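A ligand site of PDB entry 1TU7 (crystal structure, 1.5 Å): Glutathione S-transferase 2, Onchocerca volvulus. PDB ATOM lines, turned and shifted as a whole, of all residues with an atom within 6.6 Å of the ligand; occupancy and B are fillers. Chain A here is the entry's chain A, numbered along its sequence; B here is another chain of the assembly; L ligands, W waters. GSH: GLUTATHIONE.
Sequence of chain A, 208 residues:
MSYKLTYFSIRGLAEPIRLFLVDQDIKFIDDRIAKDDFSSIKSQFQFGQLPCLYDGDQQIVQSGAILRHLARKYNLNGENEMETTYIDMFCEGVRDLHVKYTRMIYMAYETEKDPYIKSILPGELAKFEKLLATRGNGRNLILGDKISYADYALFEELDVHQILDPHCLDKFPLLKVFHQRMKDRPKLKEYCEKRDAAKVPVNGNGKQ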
ATOM      1  N   TYR A   7     -10.527 -10.778 -32.574  1.00  0.00           N
ATOM      2  CA  TYR A   7     -10.990 -12.153 -32.444  1.00  0.00           C
ATOM      3  C   TYR A   7     -12.079 -12.378 -33.478  1.00  0.00           C
ATOM      4  O   TYR A   7     -12.488 -11.473 -34.190  1.00  0.00           O
ATOM      5  CB  TYR A   7     -11.535 -12.432 -31.031  1.00  0.00           C
ATOM      6  CG  TYR A   7     -11.751 -13.892 -30.712  1.00  0.00           C
ATOM      7  CD1 TYR A   7     -13.030 -14.386 -30.451  1.00  0.00           C
ATOM      8  CD2 TYR A   7     -10.703 -14.794 -30.697  1.00  0.00           C
ATOM      9  CE1 TYR A   7     -13.255 -15.713 -30.169  1.00  0.00           C
ATOM     10  CE2 TYR A   7     -10.912 -16.135 -30.394  1.00  0.00           C
ATOM     11  CZ  TYR A   7     -12.199 -16.585 -30.115  1.00  0.00           C
ATOM     12  OH  TYR A   7     -12.452 -17.894 -29.810  1.00  0.00           O
ATOM     13  N   PHE A   8     -12.553 -13.606 -33.563  1.00  0.00           N
ATOM     14  CA  PHE A   8     -13.695 -13.890 -34.417  1.00  0.00           C
ATOM     15  C   PHE A   8     -14.970 -13.275 -33.840  1.00  0.00           C
ATOM     16  O   PHE A   8     -15.010 -12.795 -32.689  1.00  0.00           O
ATOM     17  CB  PHE A   8     -13.781 -15.408 -34.591  1.00  0.00           C
ATOM     18  CG  PHE A   8     -12.535 -15.978 -35.205  1.00  0.00           C
ATOM     19  CD1 PHE A   8     -11.581 -16.627 -34.437  1.00  0.00           C
ATOM     20  CD2 PHE A   8     -12.277 -15.762 -36.551  1.00  0.00           C
ATOM     21  CE1 PHE A   8     -10.404 -17.104 -34.987  1.00  0.00           C
ATOM     22  CE2 PHE A   8     -11.102 -16.227 -37.120  1.00  0.00           C
ATOM     23  CZ  PHE A   8     -10.151 -16.912 -36.332  1.00  0.00           C
ATOM     24  N   ILE A  10     -17.590 -14.176 -32.429  1.00  0.00           N
ATOM     25  CA  ILE A  10     -18.246 -15.109 -31.524  1.00  0.00           C
ATOM     26  C   ILE A  10     -17.699 -14.771 -30.144  1.00  0.00           C
ATOM     27  O   ILE A  10     -16.728 -14.032 -30.005  1.00  0.00           O
ATOM     28  CB  ILE A  10     -17.897 -16.605 -31.848  1.00  0.00           C
ATOM     29  CG1 ILE A  10     -16.422 -16.873 -31.635  1.00  0.00           C
ATOM     30  CG2 ILE A  10     -18.368 -16.975 -33.251  1.00  0.00           C
ATOM     31  CD1 ILE A  10     -15.990 -18.332 -31.707  1.00  0.00           C
ATOM     32  N   GLY A  12     -16.538 -17.216 -27.642  1.00  0.00           N
ATOM     33  CA  GLY A  12     -15.327 -17.999 -27.614  1.00  0.00           C
ATOM     34  C   GLY A  12     -14.340 -17.593 -26.551  1.00  0.00           C
ATOM     35  O   GLY A  12     -14.707 -17.311 -25.413  1.00  0.00           O
ATOM     36  N   LEU A  13     -13.061 -17.588 -26.909  1.00  0.00           N
ATOM     37  CA  LEU A  13     -11.979 -17.297 -25.975  1.00  0.00           C
ATOM     38  C   LEU A  13     -11.827 -15.851 -25.652  1.00  0.00           C
ATOM     39  O   LEU A  13     -11.188 -15.507 -24.659  1.00  0.00           O
ATOM     40  CB  LEU A  13     -10.651 -17.779 -26.565  1.00  0.00           C
ATOM     41  CG  LEU A  13     -10.537 -19.269 -26.817  1.00  0.00           C
ATOM     42  CD1 LEU A  13      -9.223 -19.545 -27.505  1.00  0.00           C
ATOM     43  CD2 LEU A  13     -10.669 -20.065 -25.526  1.00  0.00           C
ATOM     44  N   PHE A  38      -9.432 -14.376 -42.034  1.00  0.00           N
ATOM     45  CA  PHE A  38      -8.323 -14.640 -41.134  1.00  0.00           C
ATOM     46  C   PHE A  38      -7.053 -15.106 -41.856  1.00  0.00           C
ATOM     47  O   PHE A  38      -5.947 -14.677 -41.500  1.00  0.00           O
ATOM     48  CB  PHE A  38      -8.698 -15.641 -40.039  1.00  0.00           C
ATOM     49  CG  PHE A  38      -7.620 -15.810 -39.024  1.00  0.00           C
ATOM     50  CD1 PHE A  38      -7.118 -14.710 -38.362  1.00  0.00           C
ATOM     51  CD2 PHE A  38      -7.066 -17.058 -38.752  1.00  0.00           C
ATOM     52  CE1 PHE A  38      -6.071 -14.829 -37.462  1.00  0.00           C
ATOM     53  CE2 PHE A  38      -6.017 -17.188 -37.833  1.00  0.00           C
ATOM     54  CZ  PHE A  38      -5.537 -16.068 -37.187  1.00  0.00           C
ATOM     55  N   LYS A  42      -3.205 -14.129 -40.793  1.00  0.00           N
ATOM     56  CA  LYS A  42      -2.800 -15.119 -39.770  1.00  0.00           C
ATOM     57  C   LYS A  42      -1.329 -15.020 -39.367  1.00  0.00           C
ATOM     58  O   LYS A  42      -0.978 -15.172 -38.195  1.00  0.00           O
ATOM     59  CB  LYS A  42      -3.134 -16.520 -40.288  1.00  0.00           C
ATOM     60  CG  LYS A  42      -2.733 -17.651 -39.415  1.00  0.00           C
ATOM     61  CD  LYS A  42      -2.867 -18.985 -40.156  1.00  0.00           C
ATOM     62  CE  LYS A  42      -2.504 -20.167 -39.247  1.00  0.00           C
ATOM     63  NZ  LYS A  42      -3.426 -20.442 -38.061  1.00  0.00           N
ATOM     64  N   PHE A  47       1.371 -16.980 -32.783  1.00  0.00           N
ATOM     65  CA  PHE A  47       1.046 -18.392 -32.960  1.00  0.00           C
ATOM     66  C   PHE A  47       0.027 -18.663 -34.052  1.00  0.00           C
ATOM     67  O   PHE A  47      -0.543 -19.725 -34.124  1.00  0.00           O
ATOM     68  CB  PHE A  47       0.623 -19.024 -31.627  1.00  0.00           C
ATOM     69  CG  PHE A  47       1.683 -18.925 -30.577  1.00  0.00           C
ATOM     70  CD1 PHE A  47       1.604 -18.023 -29.520  1.00  0.00           C
ATOM     71  CD2 PHE A  47       2.811 -19.718 -30.704  1.00  0.00           C
ATOM     72  CE1 PHE A  47       2.630 -17.960 -28.605  1.00  0.00           C
ATOM     73  CE2 PHE A  47       3.785 -19.692 -29.838  1.00  0.00           C
ATOM     74  CZ  PHE A  47       3.744 -18.758 -28.791  1.00  0.00           C
ATOM     75  N   GLY A  48      -0.210 -17.666 -34.904  1.00  0.00           N
ATOM     76  CA  GLY A  48      -1.161 -17.797 -35.996  1.00  0.00           C
ATOM     77  C   GLY A  48      -2.603 -17.892 -35.555  1.00  0.00           C
ATOM     78  O   GLY A  48      -3.452 -18.391 -36.289  1.00  0.00           O
ATOM     79  N   GLN A  49      -2.886 -17.410 -34.340  1.00  0.00           N
ATOM     80  CA  GLN A  49      -4.205 -17.563 -33.726  1.00  0.00           C
ATOM     81  C   GLN A  49      -4.640 -16.290 -32.982  1.00  0.00           C
ATOM     82  O   GLN A  49      -3.862 -15.364 -32.732  1.00  0.00           O
ATOM     83  CB  GLN A  49      -4.192 -18.778 -32.773  1.00  0.00           C
ATOM     84  CG  GLN A  49      -4.034 -20.102 -33.545  1.00  0.00           C
ATOM     85  CD  GLN A  49      -4.523 -21.304 -32.793  1.00  0.00           C
ATOM     86  OE1 GLN A  49      -5.356 -22.089 -33.315  1.00  0.00           O
ATOM     87  NE2 GLN A  49      -4.063 -21.461 -31.584  1.00  0.00           N
ATOM     88  N   LEU A  50      -5.923 -16.252 -32.687  1.00  0.00           N
ATOM     89  CA  LEU A  50      -6.575 -15.173 -31.955  1.00  0.00           C
ATOM     90  C   LEU A  50      -7.116 -15.763 -30.650  1.00  0.00           C
ATOM     91  O   LEU A  50      -7.345 -16.968 -30.563  1.00  0.00           O
ATOM     92  CB  LEU A  50      -7.718 -14.599 -32.807  1.00  0.00           C
ATOM     93  CG  LEU A  50      -7.280 -14.048 -34.166  1.00  0.00           C
ATOM     94  CD1 LEU A  50      -8.473 -13.496 -34.952  1.00  0.00           C
ATOM     95  CD2 LEU A  50      -6.203 -13.003 -34.038  1.00  0.00           C
ATOM     96  N   PRO A  51      -7.392 -14.968 -29.606  1.00  0.00           N
ATOM     97  CA  PRO A  51      -7.416 -13.510 -29.626  1.00  0.00           C
ATOM     98  C   PRO A  51      -6.077 -12.842 -29.565  1.00  0.00           C
ATOM     99  O   PRO A  51      -5.081 -13.469 -29.168  1.00  0.00           O
ATOM    100  CB  PRO A  51      -8.212 -13.189 -28.344  1.00  0.00           C
ATOM    101  CG  PRO A  51      -7.915 -14.310 -27.437  1.00  0.00           C
ATOM    102  CD  PRO A  51      -7.874 -15.507 -28.329  1.00  0.00           C
ATOM    103  N   VAL A  61      -0.771 -11.929 -27.898  1.00  0.00           N
ATOM    104  CA  VAL A  61      -1.659 -13.051 -28.088  1.00  0.00           C
ATOM    105  C   VAL A  61      -1.645 -13.942 -26.835  1.00  0.00           C
ATOM    106  O   VAL A  61      -0.923 -13.637 -25.869  1.00  0.00           O
ATOM    107  CB  VAL A  61      -1.347 -13.849 -29.391  1.00  0.00           C
ATOM    108  CG1 VAL A  61      -1.574 -12.972 -30.604  1.00  0.00           C
ATOM    109  CG2 VAL A  61       0.060 -14.437 -29.406  1.00  0.00           C
ATOM    110  N   GLN A  62      -2.489 -14.982 -26.848  1.00  0.00           N
ATOM    111  CA  GLN A  62      -2.734 -15.922 -25.754  1.00  0.00           C
ATOM    112  C   GLN A  62      -3.689 -15.316 -24.759  1.00  0.00           C
ATOM    113  O   GLN A  62      -3.334 -14.447 -23.981  1.00  0.00           O
ATOM    114  CB  GLN A  62      -1.449 -16.442 -25.101  1.00  0.00           C
ATOM    115  CG  GLN A  62      -0.652 -17.354 -26.026  1.00  0.00           C
ATOM    116  CD  GLN A  62      -1.259 -18.717 -26.259  1.00  0.00           C
ATOM    117  OE1 GLN A  62      -0.784 -19.476 -27.149  1.00  0.00           O
ATOM    118  NE2 GLN A  62      -2.247 -19.063 -25.499  1.00  0.00           N
ATOM    119  N   SER A  63      -4.915 -15.829 -24.753  1.00  0.00           N
ATOM    120  CA  SER A  63      -5.974 -15.281 -23.945  1.00  0.00           C
ATOM    121  C   SER A  63      -5.588 -15.159 -22.486  1.00  0.00           C
ATOM    122  O   SER A  63      -5.924 -14.170 -21.860  1.00  0.00           O
ATOM    123  CB  SER A  63      -7.257 -16.086 -24.098  1.00  0.00           C
ATOM    124  OG  SER A  63      -7.122 -17.429 -23.643  1.00  0.00           O
ATOM    125  N   GLY A  64      -4.902 -16.155 -21.915  1.00  0.00           N
ATOM    126  CA  GLY A  64      -4.525 -16.045 -20.520  1.00  0.00           C
ATOM    127  C   GLY A  64      -3.489 -14.992 -20.240  1.00  0.00           C
ATOM    128  O   GLY A  64      -3.502 -14.305 -19.218  1.00  0.00           O
ATOM    129  N   ILE A  66      -3.133 -12.270 -22.066  1.00  0.00           N
ATOM    130  CA  ILE A  66      -3.844 -11.013 -22.246  1.00  0.00           C
ATOM    131  C   ILE A  66      -4.558 -10.644 -20.954  1.00  0.00           C
ATOM    132  O   ILE A  66      -4.451  -9.523 -20.457  1.00  0.00           O
ATOM    133  CB  ILE A  66      -4.855 -11.108 -23.431  1.00  0.00           C
ATOM    134  CG1 ILE A  66      -4.141 -11.275 -24.773  1.00  0.00           C
ATOM    135  CG2 ILE A  66      -5.774  -9.882 -23.428  1.00  0.00           C
ATOM    136  CD1 ILE A  66      -5.039 -11.725 -25.914  1.00  0.00           C
ATOM    137  N   ARG A  95     -10.747 -22.686 -17.328  1.00  0.00           N
ATOM    138  CA  ARG A  95     -10.274 -23.024 -18.681  1.00  0.00           C
ATOM    139  C   ARG A  95     -10.368 -24.525 -18.934  1.00  0.00           C
ATOM    140  O   ARG A  95     -10.720 -24.941 -20.055  1.00  0.00           O
ATOM    141  CB  ARG A  95      -8.867 -22.504 -18.877  1.00  0.00           C
ATOM    142  CG  ARG A  95      -8.830 -21.015 -18.964  1.00  0.00           C
ATOM    143  CD  ARG A  95      -7.456 -20.448 -18.847  1.00  0.00           C
ATOM    144  NE  ARG A  95      -6.672 -20.700 -20.038  1.00  0.00           N
ATOM    145  CZ  ARG A  95      -6.519 -19.822 -21.048  1.00  0.00           C
ATOM    146  NH1 ARG A  95      -7.111 -18.637 -21.044  1.00  0.00           N
ATOM    147  NH2 ARG A  95      -5.772 -20.176 -22.088  1.00  0.00           N
ATOM    148  N   TYR A 106     -17.708 -28.883 -30.497  1.00  0.00           N
ATOM    149  CA  TYR A 106     -17.112 -28.892 -31.845  1.00  0.00           C
ATOM    150  C   TYR A 106     -16.979 -30.312 -32.389  1.00  0.00           C
ATOM    151  O   TYR A 106     -16.938 -30.473 -33.612  1.00  0.00           O
ATOM    152  CB  TYR A 106     -15.750 -28.187 -31.890  1.00  0.00           C
ATOM    153  CG  TYR A 106     -15.851 -26.678 -31.802  1.00  0.00           C
ATOM    154  CD1 TYR A 106     -15.640 -26.027 -30.603  1.00  0.00           C
ATOM    155  CD2 TYR A 106     -16.131 -25.879 -32.919  1.00  0.00           C
ATOM    156  CE1 TYR A 106     -15.733 -24.660 -30.488  1.00  0.00           C
ATOM    157  CE2 TYR A 106     -16.225 -24.492 -32.812  1.00  0.00           C
ATOM    158  CZ  TYR A 106     -16.032 -23.892 -31.570  1.00  0.00           C
ATOM    159  OH  TYR A 106     -16.101 -22.510 -31.442  1.00  0.00           O
ATOM    160  N   GLU B  92       2.447 -19.992 -22.639  1.00  0.00           N
ATOM    161  CA  GLU B  92       1.123 -20.459 -23.064  1.00  0.00           C
ATOM    162  C   GLU B  92       1.162 -21.061 -24.454  1.00  0.00           C
ATOM    163  O   GLU B  92       0.441 -22.009 -24.724  1.00  0.00           O
ATOM    164  CB  GLU B  92       0.113 -19.322 -23.028  1.00  0.00           C
ATOM    165  CG  GLU B  92      -0.232 -18.870 -21.618  1.00  0.00           C
ATOM    166  CD  GLU B  92      -1.066 -19.888 -20.884  1.00  0.00           C
ATOM    167  OE1 GLU B  92      -2.245 -20.027 -21.249  1.00  0.00           O
ATOM    168  OE2 GLU B  92      -0.544 -20.552 -19.974  1.00  0.00           O
ATOM    169  N   GLY B  93       2.012 -20.549 -25.328  1.00  0.00           N
ATOM    170  CA  GLY B  93       2.175 -21.189 -26.618  1.00  0.00           C
ATOM    171  C   GLY B  93       2.791 -22.579 -26.488  1.00  0.00           C
ATOM    172  O   GLY B  93       2.417 -23.498 -27.205  1.00  0.00           O
ATOM    173  N   ASP B  96       0.093 -24.936 -25.635  1.00  0.00           N
ATOM    174  CA  ASP B  96      -0.739 -25.293 -26.784  1.00  0.00           C
ATOM    175  C   ASP B  96      -0.055 -26.410 -27.596  1.00  0.00           C
ATOM    176  O   ASP B  96      -0.710 -27.361 -28.034  1.00  0.00           O
ATOM    177  CB  ASP B  96      -0.947 -24.119 -27.720  1.00  0.00           C
ATOM    178  CG  ASP B  96      -2.014 -23.165 -27.252  1.00  0.00           C
ATOM    179  OD1 ASP B  96      -2.835 -23.529 -26.401  1.00  0.00           O
ATOM    180  OD2 ASP B  96      -2.034 -22.005 -27.668  1.00  0.00           O
ATOM    181  N   LYS B 127       6.871 -21.428 -35.522  1.00  0.00           N
ATOM    182  CA  LYS B 127       6.352 -20.280 -34.799  1.00  0.00           C
ATOM    183  C   LYS B 127       7.282 -19.947 -33.654  1.00  0.00           C
ATOM    184  O   LYS B 127       7.579 -18.759 -33.416  1.00  0.00           O
ATOM    185  CB  LYS B 127       4.913 -20.523 -34.307  1.00  0.00           C
ATOM    186  CG  LYS B 127       3.907 -20.594 -35.429  1.00  0.00           C
ATOM    187  CD  LYS B 127       2.603 -21.270 -35.024  1.00  0.00           C
ATOM    188  CE  LYS B 127       1.605 -21.203 -36.142  1.00  0.00           C
ATOM    189  NZ  LYS B 127       0.372 -22.020 -35.890  1.00  0.00           N
HETATM  190  N1  GSH L   1      -4.213 -20.994 -26.163  1.00  0.00           N
HETATM  191  CA1 GSH L   1      -4.857 -20.120 -27.068  1.00  0.00           C
HETATM  192  C1  GSH L   1      -5.396 -18.915 -26.428  1.00  0.00           C
HETATM  193  O11 GSH L   1      -5.932 -19.143 -25.207  1.00  0.00           O
HETATM  194  O12 GSH L   1      -5.513 -17.714 -26.866  1.00  0.00           O
HETATM  195  CB1 GSH L   1      -5.736 -20.627 -28.126  1.00  0.00           C
HETATM  196  CG1 GSH L   1      -6.022 -19.735 -29.312  1.00  0.00           C
HETATM  197  CD1 GSH L   1      -6.922 -20.436 -30.318  1.00  0.00           C
HETATM  198  OE1 GSH L   1      -7.157 -21.761 -30.166  1.00  0.00           O
HETATM  199  N2  GSH L   1      -7.449 -19.718 -31.263  1.00  0.00           N
HETATM  200  CA2 GSH L   1      -8.385 -20.250 -32.261  1.00  0.00           C
HETATM  201  C2  GSH L   1      -8.014 -19.713 -33.586  1.00  0.00           C
HETATM  202  O2  GSH L   1      -7.370 -18.498 -33.701  1.00  0.00           O
HETATM  203  CB2 GSH L   1      -9.807 -19.784 -31.967  1.00  0.00           C
HETATM  204  SG2 GSH L   1     -10.506 -20.652 -30.543  1.00  0.00           S
HETATM  205  N3  GSH L   1      -8.290 -20.421 -34.669  1.00  0.00           N
HETATM  206  CA3 GSH L   1      -7.944 -19.864 -35.946  1.00  0.00           C
HETATM  207  C3  GSH L   1      -6.950 -20.739 -36.653  1.00  0.00           C
HETATM  208  O31 GSH L   1      -6.081 -21.519 -36.057  1.00  0.00           O
HETATM  209  O32 GSH L   1      -6.991 -20.689 -38.059  1.00  0.00           O
HETATM  210  O   HOH W   1      -3.514 -18.413 -22.986  1.00  0.00           O
HETATM  211  O   HOH W   2     -12.694 -22.790 -31.679  1.00  0.00           O
HETATM  212  O   HOH W   3      -6.398 -22.738 -25.340  1.00  0.00           O
HETATM  213  O   HOH W   4      -8.358 -23.732 -34.532  1.00  0.00           O
HETATM  214  O   HOH W   5      -8.261 -23.389 -27.948  1.00  0.00           O
HETATM  215  O   HOH W   6      -9.214 -20.255 -39.556  1.00  0.00           O
HETATM  216  O   HOH W   7      -6.076 -24.172 -30.855  1.00  0.00           O
HETATM  217  O   HOH W   8      -4.331 -16.131 -28.773  1.00  0.00           O
HETATM  218  O   HOH W   9      -2.519 -21.908 -23.897  1.00  0.00           O
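Phe 8 touches the ligand.
Leu 13 touches the ligand (CD1 to SG2, 3.5 Å).
Phe 38 touches the ligand (CE2 to O32, 3.6 Å).
Pro 51 touches the ligand.
Hydrophobic or aromatic side chains within 4 Å of the ligand: Phe 8, Leu 13, Phe 38 and Pro 51.
12 residues have an atom within 4 Å of the ligand: Tyr 7, Phe 8, Leu 13, Phe 38, Lys 42, Gln 49, Leu 50, Pro 51, Gln 62, Ser 63, Arg 95 and Asp 96 of chain B.
The nearest printed residue that does not touch the ligand is Gly 48 (4.1 Å).
Water W7 bridges an oxygen (OE1) of the ligand (2.7 Å) and the side-chain amide oxygen (OE1) of Gln 49 (3.3 Å).
Water W8 lies within hydrogen-bond range of an oxygen (O12) of the ligand (2.7 Å), the backbone carbonyl oxygen of Pro 51 (2.8 Å) and the backbone NH of Gln 62 (2.9 Å).
Water W9 lies within hydrogen-bond range of a nitrogen (N1) of the ligand (3.0 Å), the side-chain carboxylate (OD1) of Asp 96 of chain B (3.0 Å), the backbone carbonyl oxygen (O) of Glu 92 of chain B (3.1 Å) and the side-chain amide nitrogen (NE2) of Gln 62 (3.3 Å).
Water W2 lies within hydrogen-bond range of a sulfur (SG2) of the ligand (3.3 Å) and the side-chain hydroxyl of Tyr 106 (3.4 Å).
The side-chain hydroxyl (OH) of Tyr 7 sits at hydrogen-bond distance from the backbone NH (N) of Leu 13 (3.0 Å).
The side-chain carboxylate (OE1) of Glu 92 of chain B is in salt-bridge range of the guanidinium group (NH2) of Arg 95, at 3.6 Å.
The side-chain carboxylate of Asp 96 of chain B sits close to the side-chain amide oxygen of Gln 62 (2.9 Å).
The side-chain hydroxyl (OG) of Ser 63 is in hydrogen-bond range of the guanidinium group (NH1) of Arg 95 (2.9 Å).
The side-chain amino group of Lys 42 sits at hydrogen-bond distance from the backbone carbonyl oxygen of Gly 48, at 2.7 Å.
O31 of the ligand is in salt-bridge range of NZ of Lys 42.
A nitrogen (N2) of the ligand lies within hydrogen-bond range of the backbone carbonyl oxygen of Leu 50 (2.8 Å).
The side-chain hydroxyl of Ser 63 lies within hydrogen-bond range of an oxygen (O11) of the ligand, at 2.6 Å.
The side-chain hydroxyl (OH) of Tyr 7 lies close to a sulfur (SG2) of the ligand, at 3.5 Å.
OE1 of Gln 49 lies close to O31 of the ligand, at 2.9 Å.
N1 of the ligand is in salt-bridge range of OD2 of Asp 96 of chain B, at 2.8 Å.
O2 of the ligand sits at hydrogen-bond distance from N of Leu 50.
The backbone NH of Ser 63 sits at hydrogen-bond distance from an oxygen (O12) of the ligand.
NH2 of Arg 95 is in salt-bridge range of O11 of the ligand (3.3 Å).
NE2 of Gln 62 sits close to N1 of the ligand (2.8 Å).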
